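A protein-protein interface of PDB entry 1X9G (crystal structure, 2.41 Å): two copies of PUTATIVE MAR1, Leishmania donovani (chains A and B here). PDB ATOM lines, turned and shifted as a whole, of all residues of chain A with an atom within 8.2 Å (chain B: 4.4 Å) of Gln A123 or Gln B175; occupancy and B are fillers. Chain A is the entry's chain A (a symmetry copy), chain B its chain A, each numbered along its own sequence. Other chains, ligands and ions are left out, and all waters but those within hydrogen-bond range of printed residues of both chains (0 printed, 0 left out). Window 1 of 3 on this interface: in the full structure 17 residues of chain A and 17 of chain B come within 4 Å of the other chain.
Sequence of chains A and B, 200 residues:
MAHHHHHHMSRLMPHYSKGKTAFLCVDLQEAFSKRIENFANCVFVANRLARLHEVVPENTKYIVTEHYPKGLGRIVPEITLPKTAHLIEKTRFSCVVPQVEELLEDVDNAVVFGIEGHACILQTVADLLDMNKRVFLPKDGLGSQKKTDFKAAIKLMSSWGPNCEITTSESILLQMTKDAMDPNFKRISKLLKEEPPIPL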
ATOM      1  N   ARG A  92     -13.959 -24.869  -5.445  1.00  0.00           N
ATOM      2  CA  ARG A  92     -14.349 -25.023  -6.835  1.00  0.00           C
ATOM      3  C   ARG A  92     -15.254 -23.849  -7.260  1.00  0.00           C
ATOM      4  O   ARG A  92     -16.157 -23.458  -6.493  1.00  0.00           O
ATOM      5  CB  ARG A  92     -15.024 -26.376  -7.013  1.00  0.00           C
ATOM      6  CG  ARG A  92     -15.633 -26.644  -8.366  1.00  0.00           C
ATOM      7  CD  ARG A  92     -15.363 -28.069  -8.772  1.00  0.00           C
ATOM      8  NE  ARG A  92     -14.184 -28.099  -9.640  1.00  0.00           N
ATOM      9  CZ  ARG A  92     -14.158 -28.576 -10.883  1.00  0.00           C
ATOM     10  NH1 ARG A  92     -15.256 -29.088 -11.437  1.00  0.00           N
ATOM     11  NH2 ARG A  92     -13.016 -28.554 -11.569  1.00  0.00           N
ATOM     12  N   PHE A  93     -14.984 -23.248  -8.434  1.00  0.00           N
ATOM     13  CA  PHE A  93     -15.805 -22.100  -8.884  1.00  0.00           C
ATOM     14  C   PHE A  93     -17.216 -22.579  -9.174  1.00  0.00           C
ATOM     15  O   PHE A  93     -18.188 -21.956  -8.749  1.00  0.00           O
ATOM     16  CB  PHE A  93     -15.195 -21.314 -10.048  1.00  0.00           C
ATOM     17  CG  PHE A  93     -13.889 -20.681  -9.720  1.00  0.00           C
ATOM     18  CD1 PHE A  93     -12.803 -20.798 -10.588  1.00  0.00           C
ATOM     19  CD2 PHE A  93     -13.717 -19.998  -8.504  1.00  0.00           C
ATOM     20  CE1 PHE A  93     -11.552 -20.213 -10.263  1.00  0.00           C
ATOM     21  CE2 PHE A  93     -12.469 -19.427  -8.152  1.00  0.00           C
ATOM     22  CZ  PHE A  93     -11.384 -19.530  -9.055  1.00  0.00           C
ATOM     23  N   SER A  94     -17.318 -23.725  -9.830  1.00  0.00           N
ATOM     24  CA  SER A  94     -18.587 -24.411  -9.967  1.00  0.00           C
ATOM     25  C   SER A  94     -19.115 -25.105  -8.716  1.00  0.00           C
ATOM     26  O   SER A  94     -18.363 -25.831  -8.040  1.00  0.00           O
ATOM     27  CB  SER A  94     -18.450 -25.484 -11.006  1.00  0.00           C
ATOM     28  OG  SER A  94     -19.624 -26.243 -10.974  1.00  0.00           O
ATOM     29  N   CYS A  95     -20.414 -24.912  -8.455  1.00  0.00           N
ATOM     30  CA  CYS A  95     -21.205 -25.648  -7.465  1.00  0.00           C
ATOM     31  C   CYS A  95     -21.207 -27.161  -7.581  1.00  0.00           C
ATOM     32  O   CYS A  95     -21.495 -27.836  -6.601  1.00  0.00           O
ATOM     33  CB  CYS A  95     -22.667 -25.209  -7.478  1.00  0.00           C
ATOM     34  SG  CYS A  95     -22.946 -23.520  -6.912  1.00  0.00           S
ATOM     35  N   VAL A  96     -20.882 -27.720  -8.737  1.00  0.00           N
ATOM     36  CA  VAL A  96     -20.865 -29.184  -8.852  1.00  0.00           C
ATOM     37  C   VAL A  96     -19.615 -29.789  -8.181  1.00  0.00           C
ATOM     38  O   VAL A  96     -18.577 -30.038  -8.815  1.00  0.00           O
ATOM     39  CB  VAL A  96     -21.076 -29.660 -10.306  1.00  0.00           C
ATOM     40  CG1 VAL A  96     -21.284 -31.173 -10.359  1.00  0.00           C
ATOM     41  CG2 VAL A  96     -22.284 -28.911 -10.935  1.00  0.00           C
ATOM     42  N   VAL A 112     -31.252 -22.267 -10.751  1.00  0.00           N
ATOM     43  CA  VAL A 112     -29.952 -21.782 -10.303  1.00  0.00           C
ATOM     44  C   VAL A 112     -29.992 -20.282 -10.170  1.00  0.00           C
ATOM     45  O   VAL A 112     -30.447 -19.602 -11.063  1.00  0.00           O
ATOM     46  CB  VAL A 112     -28.847 -22.227 -11.254  1.00  0.00           C
ATOM     47  CG1 VAL A 112     -27.498 -21.751 -10.771  1.00  0.00           C
ATOM     48  CG2 VAL A 112     -28.807 -23.712 -11.328  1.00  0.00           C
ATOM     49  N   GLU A 116     -21.509 -15.269  -9.065  1.00  0.00           N
ATOM     50  CA  GLU A 116     -21.593 -14.279 -10.152  1.00  0.00           C
ATOM     51  C   GLU A 116     -21.923 -14.929 -11.475  1.00  0.00           C
ATOM     52  O   GLU A 116     -21.380 -15.995 -11.797  1.00  0.00           O
ATOM     53  CB  GLU A 116     -20.263 -13.547 -10.292  1.00  0.00           C
ATOM     54  CG  GLU A 116     -19.738 -12.923  -9.016  1.00  0.00           C
ATOM     55  CD  GLU A 116     -18.909 -11.659  -9.247  1.00  0.00           C
ATOM     56  OE1 GLU A 116     -17.936 -11.482  -8.482  1.00  0.00           O
ATOM     57  OE2 GLU A 116     -19.205 -10.846 -10.171  1.00  0.00           O
ATOM     58  N   GLY A 117     -22.761 -14.237 -12.265  1.00  0.00           N
ATOM     59  CA  GLY A 117     -23.271 -14.714 -13.570  1.00  0.00           C
ATOM     60  C   GLY A 117     -22.235 -15.344 -14.490  1.00  0.00           C
ATOM     61  O   GLY A 117     -22.477 -16.389 -15.110  1.00  0.00           O
ATOM     62  N   HIS A 118     -21.060 -14.712 -14.544  1.00  0.00           N
ATOM     63  CA  HIS A 118     -19.995 -15.104 -15.464  1.00  0.00           C
ATOM     64  C   HIS A 118     -18.939 -16.025 -14.856  1.00  0.00           C
ATOM     65  O   HIS A 118     -17.979 -16.400 -15.554  1.00  0.00           O
ATOM     66  CB  HIS A 118     -19.311 -13.855 -15.996  1.00  0.00           C
ATOM     67  CG  HIS A 118     -18.627 -13.065 -14.932  1.00  0.00           C
ATOM     68  ND1 HIS A 118     -19.325 -12.339 -13.984  1.00  0.00           N
ATOM     69  CD2 HIS A 118     -17.316 -12.929 -14.627  1.00  0.00           C
ATOM     70  CE1 HIS A 118     -18.462 -11.749 -13.168  1.00  0.00           C
ATOM     71  NE2 HIS A 118     -17.237 -12.079 -13.548  1.00  0.00           N
ATOM     72  N   ALA A 119     -19.118 -16.394 -13.580  1.00  0.00           N
ATOM     73  CA  ALA A 119     -18.074 -17.071 -12.843  1.00  0.00           C
ATOM     74  C   ALA A 119     -18.619 -18.364 -12.274  1.00  0.00           C
ATOM     75  O   ALA A 119     -18.794 -19.323 -13.023  1.00  0.00           O
ATOM     76  CB  ALA A 119     -17.485 -16.116 -11.760  1.00  0.00           C
ATOM     77  N   CYS A 120     -18.962 -18.402 -10.982  1.00  0.00           N
ATOM     78  CA  CYS A 120     -19.524 -19.592 -10.396  1.00  0.00           C
ATOM     79  C   CYS A 120     -20.793 -20.039 -11.110  1.00  0.00           C
ATOM     80  O   CYS A 120     -20.945 -21.256 -11.373  1.00  0.00           O
ATOM     81  CB  CYS A 120     -19.790 -19.389  -8.885  1.00  0.00           C
ATOM     82  SG  CYS A 120     -18.339 -18.757  -7.865  1.00  0.00           S
ATOM     83  N   ILE A 121     -21.702 -19.081 -11.419  1.00  0.00           N
ATOM     84  CA  ILE A 121     -23.037 -19.413 -12.036  1.00  0.00           C
ATOM     85  C   ILE A 121     -22.811 -20.098 -13.368  1.00  0.00           C
ATOM     86  O   ILE A 121     -23.249 -21.204 -13.594  1.00  0.00           O
ATOM     87  CB  ILE A 121     -23.978 -18.155 -12.268  1.00  0.00           C
ATOM     88  CG1 ILE A 121     -24.432 -17.479 -10.951  1.00  0.00           C
ATOM     89  CG2 ILE A 121     -25.177 -18.511 -13.131  1.00  0.00           C
ATOM     90  CD1 ILE A 121     -25.403 -18.264 -10.086  1.00  0.00           C
ATOM     91  N   LEU A 122     -22.058 -19.415 -14.219  1.00  0.00           N
ATOM     92  CA  LEU A 122     -21.687 -19.897 -15.542  1.00  0.00           C
ATOM     93  C   LEU A 122     -21.065 -21.334 -15.499  1.00  0.00           C
ATOM     94  O   LEU A 122     -21.549 -22.250 -16.151  1.00  0.00           O
ATOM     95  CB  LEU A 122     -20.801 -18.835 -16.236  1.00  0.00           C
ATOM     96  CG  LEU A 122     -20.370 -19.125 -17.690  1.00  0.00           C
ATOM     97  CD1 LEU A 122     -21.505 -18.950 -18.708  1.00  0.00           C
ATOM     98  CD2 LEU A 122     -19.167 -18.267 -18.117  1.00  0.00           C
ATOM     99  N   GLN A 123     -20.018 -21.535 -14.699  1.00  0.00           N
ATOM    100  CA  GLN A 123     -19.396 -22.884 -14.570  1.00  0.00           C
ATOM    101  C   GLN A 123     -20.340 -23.919 -14.013  1.00  0.00           C
ATOM    102  O   GLN A 123     -20.379 -25.073 -14.484  1.00  0.00           O
ATOM    103  CB  GLN A 123     -18.083 -22.829 -13.757  1.00  0.00           C
ATOM    104  CG  GLN A 123     -17.128 -21.789 -14.355  1.00  0.00           C
ATOM    105  CD  GLN A 123     -15.713 -21.867 -13.851  1.00  0.00           C
ATOM    106  OE1 GLN A 123     -15.165 -22.953 -13.695  1.00  0.00           O
ATOM    107  NE2 GLN A 123     -15.079 -20.707 -13.662  1.00  0.00           N
ATOM    108  N   THR A 124     -21.130 -23.493 -13.034  1.00  0.00           N
ATOM    109  CA  THR A 124     -22.142 -24.367 -12.411  1.00  0.00           C
ATOM    110  C   THR A 124     -23.133 -24.894 -13.459  1.00  0.00           C
ATOM    111  O   THR A 124     -23.346 -26.113 -13.546  1.00  0.00           O
ATOM    112  CB  THR A 124     -22.891 -23.581 -11.357  1.00  0.00           C
ATOM    113  OG1 THR A 124     -21.950 -23.173 -10.360  1.00  0.00           O
ATOM    114  CG2 THR A 124     -23.978 -24.371 -10.759  1.00  0.00           C
ATOM    115  N   VAL A 125     -23.697 -23.992 -14.291  1.00  0.00           N
ATOM    116  CA  VAL A 125     -24.644 -24.457 -15.299  1.00  0.00           C
ATOM    117  C   VAL A 125     -24.039 -25.327 -16.389  1.00  0.00           C
ATOM    118  O   VAL A 125     -24.667 -26.283 -16.777  1.00  0.00           O
ATOM    119  CB  VAL A 125     -25.706 -23.373 -15.845  1.00  0.00           C
ATOM    120  CG1 VAL A 125     -25.731 -22.119 -15.040  1.00  0.00           C
ATOM    121  CG2 VAL A 125     -25.541 -23.060 -17.278  1.00  0.00           C
ATOM    122  N   ALA A 126     -22.830 -25.045 -16.880  1.00  0.00           N
ATOM    123  CA  ALA A 126     -22.228 -25.954 -17.875  1.00  0.00           C
ATOM    124  C   ALA A 126     -22.080 -27.378 -17.293  1.00  0.00           C
ATOM    125  O   ALA A 126     -22.339 -28.353 -17.992  1.00  0.00           O
ATOM    126  CB  ALA A 126     -20.898 -25.411 -18.436  1.00  0.00           C
ATOM    127  N   ASP A 127     -21.704 -27.488 -16.010  1.00  0.00           N
ATOM    128  CA  ASP A 127     -21.593 -28.810 -15.309  1.00  0.00           C
ATOM    129  C   ASP A 127     -22.952 -29.527 -15.151  1.00  0.00           C
ATOM    130  O   ASP A 127     -23.091 -30.696 -15.504  1.00  0.00           O
ATOM    131  CB  ASP A 127     -20.904 -28.693 -13.939  1.00  0.00           C
ATOM    132  CG  ASP A 127     -19.389 -28.362 -14.018  1.00  0.00           C
ATOM    133  OD1 ASP A 127     -18.906 -27.772 -13.032  1.00  0.00           O
ATOM    134  OD2 ASP A 127     -18.672 -28.687 -15.009  1.00  0.00           O
ATOM    135  N   LEU A 128     -23.946 -28.814 -14.639  1.00  0.00           N
ATOM    136  CA  LEU A 128     -25.318 -29.298 -14.663  1.00  0.00           C
ATOM    137  C   LEU A 128     -25.742 -29.818 -16.031  1.00  0.00           C
ATOM    138  O   LEU A 128     -26.326 -30.901 -16.126  1.00  0.00           O
ATOM    139  CB  LEU A 128     -26.255 -28.194 -14.221  1.00  0.00           C
ATOM    140  CG  LEU A 128     -26.639 -28.050 -12.738  1.00  0.00           C
ATOM    141  CD1 LEU A 128     -25.963 -29.116 -11.816  1.00  0.00           C
ATOM    142  CD2 LEU A 128     -26.485 -26.583 -12.220  1.00  0.00           C
ATOM    143  N   LEU A 129     -25.435 -29.071 -17.107  1.00  0.00           N
ATOM    144  CA  LEU A 129     -25.853 -29.514 -18.428  1.00  0.00           C
ATOM    145  C   LEU A 129     -25.197 -30.817 -18.787  1.00  0.00           C
ATOM    146  O   LEU A 129     -25.858 -31.709 -19.288  1.00  0.00           O
ATOM    147  CB  LEU A 129     -25.652 -28.452 -19.541  1.00  0.00           C
ATOM    148  CG  LEU A 129     -26.632 -27.269 -19.501  1.00  0.00           C
ATOM    149  CD1 LEU A 129     -26.275 -26.189 -20.507  1.00  0.00           C
ATOM    150  CD2 LEU A 129     -28.121 -27.644 -19.552  1.00  0.00           C
ATOM    151  N   ASP A 130     -23.900 -30.921 -18.530  1.00  0.00           N
ATOM    152  CA  ASP A 130     -23.169 -32.181 -18.663  1.00  0.00           C
ATOM    153  C   ASP A 130     -23.714 -33.352 -17.837  1.00  0.00           C
ATOM    154  O   ASP A 130     -23.520 -34.504 -18.215  1.00  0.00           O
ATOM    155  CB  ASP A 130     -21.690 -31.962 -18.404  1.00  0.00           C
ATOM    156  CG  ASP A 130     -21.003 -31.388 -19.621  1.00  0.00           C
ATOM    157  OD1 ASP A 130     -21.018 -30.140 -19.834  1.00  0.00           O
ATOM    158  OD2 ASP A 130     -20.508 -32.209 -20.431  1.00  0.00           O
ATOM    159  N   ALA A 153     -21.992 -13.353 -20.225  1.00  0.00           N
ATOM    160  CA  ALA A 153     -22.278 -14.701 -19.706  1.00  0.00           C
ATOM    161  C   ALA A 153     -23.756 -15.058 -19.962  1.00  0.00           C
ATOM    162  O   ALA A 153     -24.077 -16.173 -20.402  1.00  0.00           O
ATOM    163  CB  ALA A 153     -21.937 -14.763 -18.231  1.00  0.00           C
ATOM    164  N   LEU A 156     -24.215 -15.969 -23.672  1.00  0.00           N
ATOM    165  CA  LEU A 156     -23.675 -17.303 -23.913  1.00  0.00           C
ATOM    166  C   LEU A 156     -24.741 -18.343 -23.487  1.00  0.00           C
ATOM    167  O   LEU A 156     -25.103 -19.236 -24.243  1.00  0.00           O
ATOM    168  CB  LEU A 156     -22.444 -17.544 -23.033  1.00  0.00           C
ATOM    169  CG  LEU A 156     -21.277 -18.262 -23.688  1.00  0.00           C
ATOM    170  CD1 LEU A 156     -20.439 -19.029 -22.643  1.00  0.00           C
ATOM    171  CD2 LEU A 156     -21.662 -19.121 -24.941  1.00  0.00           C
ATOM    172  N   MET A 157     -25.169 -18.245 -22.244  1.00  0.00           N
ATOM    173  CA  MET A 157     -26.077 -19.242 -21.686  1.00  0.00           C
ATOM    174  C   MET A 157     -27.436 -19.338 -22.432  1.00  0.00           C
ATOM    175  O   MET A 157     -27.962 -20.423 -22.539  1.00  0.00           O
ATOM    176  CB  MET A 157     -26.333 -19.000 -20.189  1.00  0.00           C
ATOM    177  CG  MET A 157     -25.106 -19.247 -19.298  1.00  0.00           C
ATOM    178  SD  MET A 157     -25.401 -19.155 -17.503  1.00  0.00           S
ATOM    179  CE  MET A 157     -25.454 -17.381 -17.189  1.00  0.00           C
ATOM    180  N   TRP A 160     -27.602 -21.940 -25.052  1.00  0.00           N
ATOM    181  CA  TRP A 160     -27.411 -23.327 -24.544  1.00  0.00           C
ATOM    182  C   TRP A 160     -28.729 -24.131 -24.437  1.00  0.00           C
ATOM    183  O   TRP A 160     -28.825 -25.061 -23.603  1.00  0.00           O
ATOM    184  CB  TRP A 160     -26.721 -23.335 -23.141  1.00  0.00           C
ATOM    185  CG  TRP A 160     -25.279 -22.920 -23.178  1.00  0.00           C
ATOM    186  CD1 TRP A 160     -24.516 -22.714 -24.316  1.00  0.00           C
ATOM    187  CD2 TRP A 160     -24.398 -22.662 -22.057  1.00  0.00           C
ATOM    188  NE1 TRP A 160     -23.245 -22.367 -23.958  1.00  0.00           N
ATOM    189  CE2 TRP A 160     -23.133 -22.345 -22.593  1.00  0.00           C
ATOM    190  CE3 TRP A 160     -24.543 -22.734 -20.647  1.00  0.00           C
ATOM    191  CZ2 TRP A 160     -22.022 -22.047 -21.787  1.00  0.00           C
ATOM    192  CZ3 TRP A 160     -23.429 -22.440 -19.839  1.00  0.00           C
ATOM    193  CH2 TRP A 160     -22.186 -22.083 -20.425  1.00  0.00           C
ATOM    194  N   LEU B  12     -17.333 -24.989 -21.842  1.00  0.00           N
ATOM    195  CA  LEU B  12     -16.518 -23.764 -21.650  1.00  0.00           C
ATOM    196  C   LEU B  12     -15.030 -24.060 -21.897  1.00  0.00           C
ATOM    197  O   LEU B  12     -14.715 -25.121 -22.424  1.00  0.00           O
ATOM    198  CB  LEU B  12     -16.744 -23.189 -20.247  1.00  0.00           C
ATOM    199  CG  LEU B  12     -18.139 -22.720 -19.843  1.00  0.00           C
ATOM    200  CD1 LEU B  12     -18.289 -22.665 -18.361  1.00  0.00           C
ATOM    201  CD2 LEU B  12     -18.410 -21.340 -20.421  1.00  0.00           C
ATOM    202  N   MET B  13     -14.125 -23.141 -21.559  1.00  0.00           N
ATOM    203  CA  MET B  13     -12.682 -23.487 -21.535  1.00  0.00           C
ATOM    204  C   MET B  13     -12.406 -24.653 -20.548  1.00  0.00           C
ATOM    205  O   MET B  13     -12.961 -24.683 -19.437  1.00  0.00           O
ATOM    206  CB  MET B  13     -11.808 -22.283 -21.169  1.00  0.00           C
ATOM    207  CG  MET B  13     -11.836 -21.200 -22.231  1.00  0.00           C
ATOM    208  SD  MET B  13     -10.386 -20.202 -22.347  1.00  0.00           S
ATOM    209  CE  MET B  13      -9.331 -21.272 -23.342  1.00  0.00           C
ATOM    210  N   PRO B  14     -11.608 -25.646 -20.972  1.00  0.00           N
ATOM    211  CA  PRO B  14     -11.236 -26.716 -20.043  1.00  0.00           C
ATOM    212  C   PRO B  14     -10.118 -26.199 -19.146  1.00  0.00           C
ATOM    213  O   PRO B  14      -9.526 -25.155 -19.488  1.00  0.00           O
ATOM    214  CB  PRO B  14     -10.729 -27.833 -20.971  1.00  0.00           C
ATOM    215  CG  PRO B  14     -10.289 -27.155 -22.215  1.00  0.00           C
ATOM    216  CD  PRO B  14     -11.014 -25.824 -22.314  1.00  0.00           C
ATOM    217  N   HIS B  15      -9.851 -26.896 -18.025  1.00  0.00           N
ATOM    218  CA  HIS B  15      -8.693 -26.619 -17.155  1.00  0.00           C
ATOM    219  C   HIS B  15      -7.433 -26.392 -17.999  1.00  0.00           C
ATOM    220  O   HIS B  15      -7.196 -27.111 -18.958  1.00  0.00           O
ATOM    221  CB  HIS B  15      -8.461 -27.713 -16.072  1.00  0.00           C
ATOM    222  CG  HIS B  15      -7.365 -27.343 -15.118  1.00  0.00           C
ATOM    223  ND1 HIS B  15      -6.073 -27.825 -15.244  1.00  0.00           N
ATOM    224  CD2 HIS B  15      -7.327 -26.432 -14.110  1.00  0.00           C
ATOM    225  CE1 HIS B  15      -5.296 -27.250 -14.340  1.00  0.00           C
ATOM    226  NE2 HIS B  15      -6.028 -26.396 -13.643  1.00  0.00           N
ATOM    227  N   THR B 167     -17.182 -14.370 -24.082  1.00  0.00           N
ATOM    228  CA  THR B 167     -17.402 -14.030 -22.666  1.00  0.00           C
ATOM    229  C   THR B 167     -16.566 -12.781 -22.396  1.00  0.00           C
ATOM    230  O   THR B 167     -16.690 -11.798 -23.112  1.00  0.00           O
ATOM    231  CB  THR B 167     -17.069 -15.203 -21.691  1.00  0.00           C
ATOM    232  OG1 THR B 167     -15.803 -15.791 -22.068  1.00  0.00           O
ATOM    233  CG2 THR B 167     -18.188 -16.313 -21.686  1.00  0.00           C
ATOM    234  N   SER B 171     -14.051 -13.909 -16.951  1.00  0.00           N
ATOM    235  CA  SER B 171     -14.703 -15.221 -17.120  1.00  0.00           C
ATOM    236  C   SER B 171     -13.714 -16.249 -17.597  1.00  0.00           C
ATOM    237  O   SER B 171     -13.685 -17.338 -17.107  1.00  0.00           O
ATOM    238  CB  SER B 171     -15.799 -15.149 -18.188  1.00  0.00           C
ATOM    239  OG  SER B 171     -16.700 -16.237 -18.014  1.00  0.00           O
ATOM    240  N   ILE B 172     -12.937 -15.904 -18.607  1.00  0.00           N
ATOM    241  CA  ILE B 172     -11.950 -16.811 -19.195  1.00  0.00           C
ATOM    242  C   ILE B 172     -10.801 -17.236 -18.252  1.00  0.00           C
ATOM    243  O   ILE B 172     -10.442 -18.427 -18.256  1.00  0.00           O
ATOM    244  CB  ILE B 172     -11.377 -16.203 -20.501  1.00  0.00           C
ATOM    245  CG1 ILE B 172     -12.383 -16.369 -21.647  1.00  0.00           C
ATOM    246  CG2 ILE B 172     -10.058 -16.871 -20.924  1.00  0.00           C
ATOM    247  CD1 ILE B 172     -11.930 -15.594 -22.944  1.00  0.00           C
ATOM    248  N   LEU B 173     -10.219 -16.306 -17.467  1.00  0.00           N
ATOM    249  CA  LEU B 173      -9.186 -16.715 -16.496  1.00  0.00           C
ATOM    250  C   LEU B 173      -9.714 -17.756 -15.503  1.00  0.00           C
ATOM    251  O   LEU B 173      -9.101 -18.780 -15.311  1.00  0.00           O
ATOM    252  CB  LEU B 173      -8.548 -15.550 -15.729  1.00  0.00           C
ATOM    253  CG  LEU B 173      -7.800 -14.400 -16.411  1.00  0.00           C
ATOM    254  CD1 LEU B 173      -6.644 -13.918 -15.541  1.00  0.00           C
ATOM    255  CD2 LEU B 173      -7.320 -14.665 -17.870  1.00  0.00           C
ATOM    256  N   LEU B 174     -10.886 -17.502 -14.941  1.00  0.00           N
ATOM    257  CA  LEU B 174     -11.602 -18.397 -14.053  1.00  0.00           C
ATOM    258  C   LEU B 174     -12.014 -19.741 -14.631  1.00  0.00           C
ATOM    259  O   LEU B 174     -12.306 -20.685 -13.885  1.00  0.00           O
ATOM    260  CB  LEU B 174     -12.862 -17.669 -13.585  1.00  0.00           C
ATOM    261  CG  LEU B 174     -12.595 -16.447 -12.701  1.00  0.00           C
ATOM    262  CD1 LEU B 174     -13.871 -15.935 -12.034  1.00  0.00           C
ATOM    263  CD2 LEU B 174     -11.514 -16.750 -11.610  1.00  0.00           C
ATOM    264  N   GLN B 175     -12.123 -19.821 -15.949  1.00  0.00           N
ATOM    265  CA  GLN B 175     -12.615 -21.027 -16.579  1.00  0.00           C
ATOM    266  C   GLN B 175     -11.442 -21.980 -16.739  1.00  0.00           C
ATOM    267  O   GLN B 175     -11.606 -23.196 -16.676  1.00  0.00           O
ATOM    268  CB  GLN B 175     -13.233 -20.716 -17.940  1.00  0.00           C
ATOM    269  CG  GLN B 175     -14.698 -20.174 -17.936  1.00  0.00           C
ATOM    270  CD  GLN B 175     -15.092 -19.678 -19.326  1.00  0.00           C
ATOM    271  OE1 GLN B 175     -14.871 -20.370 -20.302  1.00  0.00           O
ATOM    272  NE2 GLN B 175     -15.602 -18.459 -19.426  1.00  0.00           N
ATOM    273  N   MET B 176     -10.264 -21.422 -16.959  1.00  0.00           N
ATOM    274  CA  MET B 176      -9.060 -22.198 -17.069  1.00  0.00           C
ATOM    275  C   MET B 176      -8.483 -22.712 -15.707  1.00  0.00           C
ATOM    276  O   MET B 176      -7.786 -23.718 -15.700  1.00  0.00           O
ATOM    277  CB  MET B 176      -8.009 -21.381 -17.831  1.00  0.00           C
ATOM    278  CG  MET B 176      -8.260 -21.253 -19.334  1.00  0.00           C
ATOM    279  SD  MET B 176      -7.213 -19.997 -20.170  1.00  0.00           S
ATOM    280  CE  MET B 176      -5.969 -21.070 -20.925  1.00  0.00           C
ATOM    281  N   THR B 177      -8.754 -22.029 -14.587  1.00  0.00           N
ATOM    282  CA  THR B 177      -8.304 -22.487 -13.252  1.00  0.00           C
ATOM    283  C   THR B 177      -9.437 -23.006 -12.418  1.00  0.00           C
ATOM    284  O   THR B 177      -9.843 -22.326 -11.493  1.00  0.00           O
ATOM    285  CB  THR B 177      -7.725 -21.334 -12.367  1.00  0.00           C
ATOM    286  OG1 THR B 177      -8.185 -20.061 -12.820  1.00  0.00           O
ATOM    287  CG2 THR B 177      -6.196 -21.351 -12.356  1.00  0.00           C
ATOM    288  N   LYS B 178      -9.977 -24.181 -12.683  1.00  0.00           N
ATOM    289  CA  LYS B 178     -11.358 -24.400 -12.257  1.00  0.00           C
ATOM    290  C   LYS B 178     -11.681 -24.315 -10.727  1.00  0.00           C
ATOM    291  O   LYS B 178     -12.831 -24.525 -10.312  1.00  0.00           O
ATOM    292  CB  LYS B 178     -11.876 -25.667 -12.921  1.00  0.00           C
ATOM    293  CG  LYS B 178     -11.973 -25.589 -14.475  1.00  0.00           C
ATOM    294  CD  LYS B 178     -13.351 -26.153 -14.968  1.00  0.00           C
ATOM    295  CE  LYS B 178     -13.518 -26.148 -16.486  1.00  0.00           C
ATOM    296  NZ  LYS B 178     -13.567 -24.752 -17.103  1.00  0.00           N
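Among the printed residues, pairs that only touch across the chains: Arg A92 with Lys B178, Phe A93 with Leu B174, Phe A93 with Thr B177, Ala A119 with Leu B174, Leu A122 with Leu B12, Leu A122 with Ser B171, Leu A122 with Gln B175, Gln A123 with Leu B12, Gln A123 with Gln B175, Gln A123 with Lys B178, Ala A126 with Leu B12, Leu A156 with Leu B12, Leu A156 with Thr B167 and Trp A160 with Leu B12.
No position is printed for both chains.
Of the 17 pairs that touch across the chains among the printed residues, none has its exchanged pair printed and touching as well.
The backbone carbonyl oxygen (O) of His A118 lies within hydrogen-bond range of the side-chain hydroxyl (OG) of Ser B171 (2.8 Å).
The backbone NH (N) of Phe A93 is in hydrogen-bond range of the backbone carbonyl oxygen (O) of Lys B178.
O of Leu B174 sits at hydrogen-bond distance from NE2 of Gln A123 (2.8 Å).
Of the 13 printed residues of chain B, 7 touch a printed residue of chain A.
Hydrophobic or aromatic side chains of chain B that line the printed part of chain A: Leu B12 and Leu B174.
Among the printed residues, 17 pairs touch across the chains.
Gln A123 touches just these residues of chain B: Leu B12, Leu B174, Gln B175 and Lys B178.
Of chain A, only Leu A122 and Gln A123 come within 4 Å of Gln B175.
Printed residues of chain B within 4 Å of Ala A119: Leu B174.
Of the printed residues of chain B, Leu A122 touches Leu B12, Ser B171 and Gln B175.
Of the printed residues of chain B, Ala A126 touches Leu B12.
Printed residues of chain B within 4 Å of Arg A92: Lys B178.
Of the printed residues of chain A, Thr B177 touches Phe A93.
Val A112 touches none of the printed residues of chain B.
The nearest printed residue of chain B that does not touch Gln A123 is Ser B171 (5.0 Å).
NE2 of Gln B175 sits at hydrogen-bond distance from OG of Ser B171, 2.9 Å away.
The side-chain amino group (NZ) of Lys B178 sits at hydrogen-bond distance from the backbone carbonyl oxygen (O) of Met B13 (2.4 Å).
N of Met B13 is in hydrogen-bond range of OE1 of Gln B175 (3.1 Å).
The backbone carbonyl oxygen (O) of Leu B173 sits at hydrogen-bond distance from the side-chain hydroxyl (OG1) of Thr B177.
N of Leu A122 sits close to O of Gly A117 (3.2 Å).
NZ of Lys B178 sits at hydrogen-bond distance from O of Gln B175 (2.5 Å).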
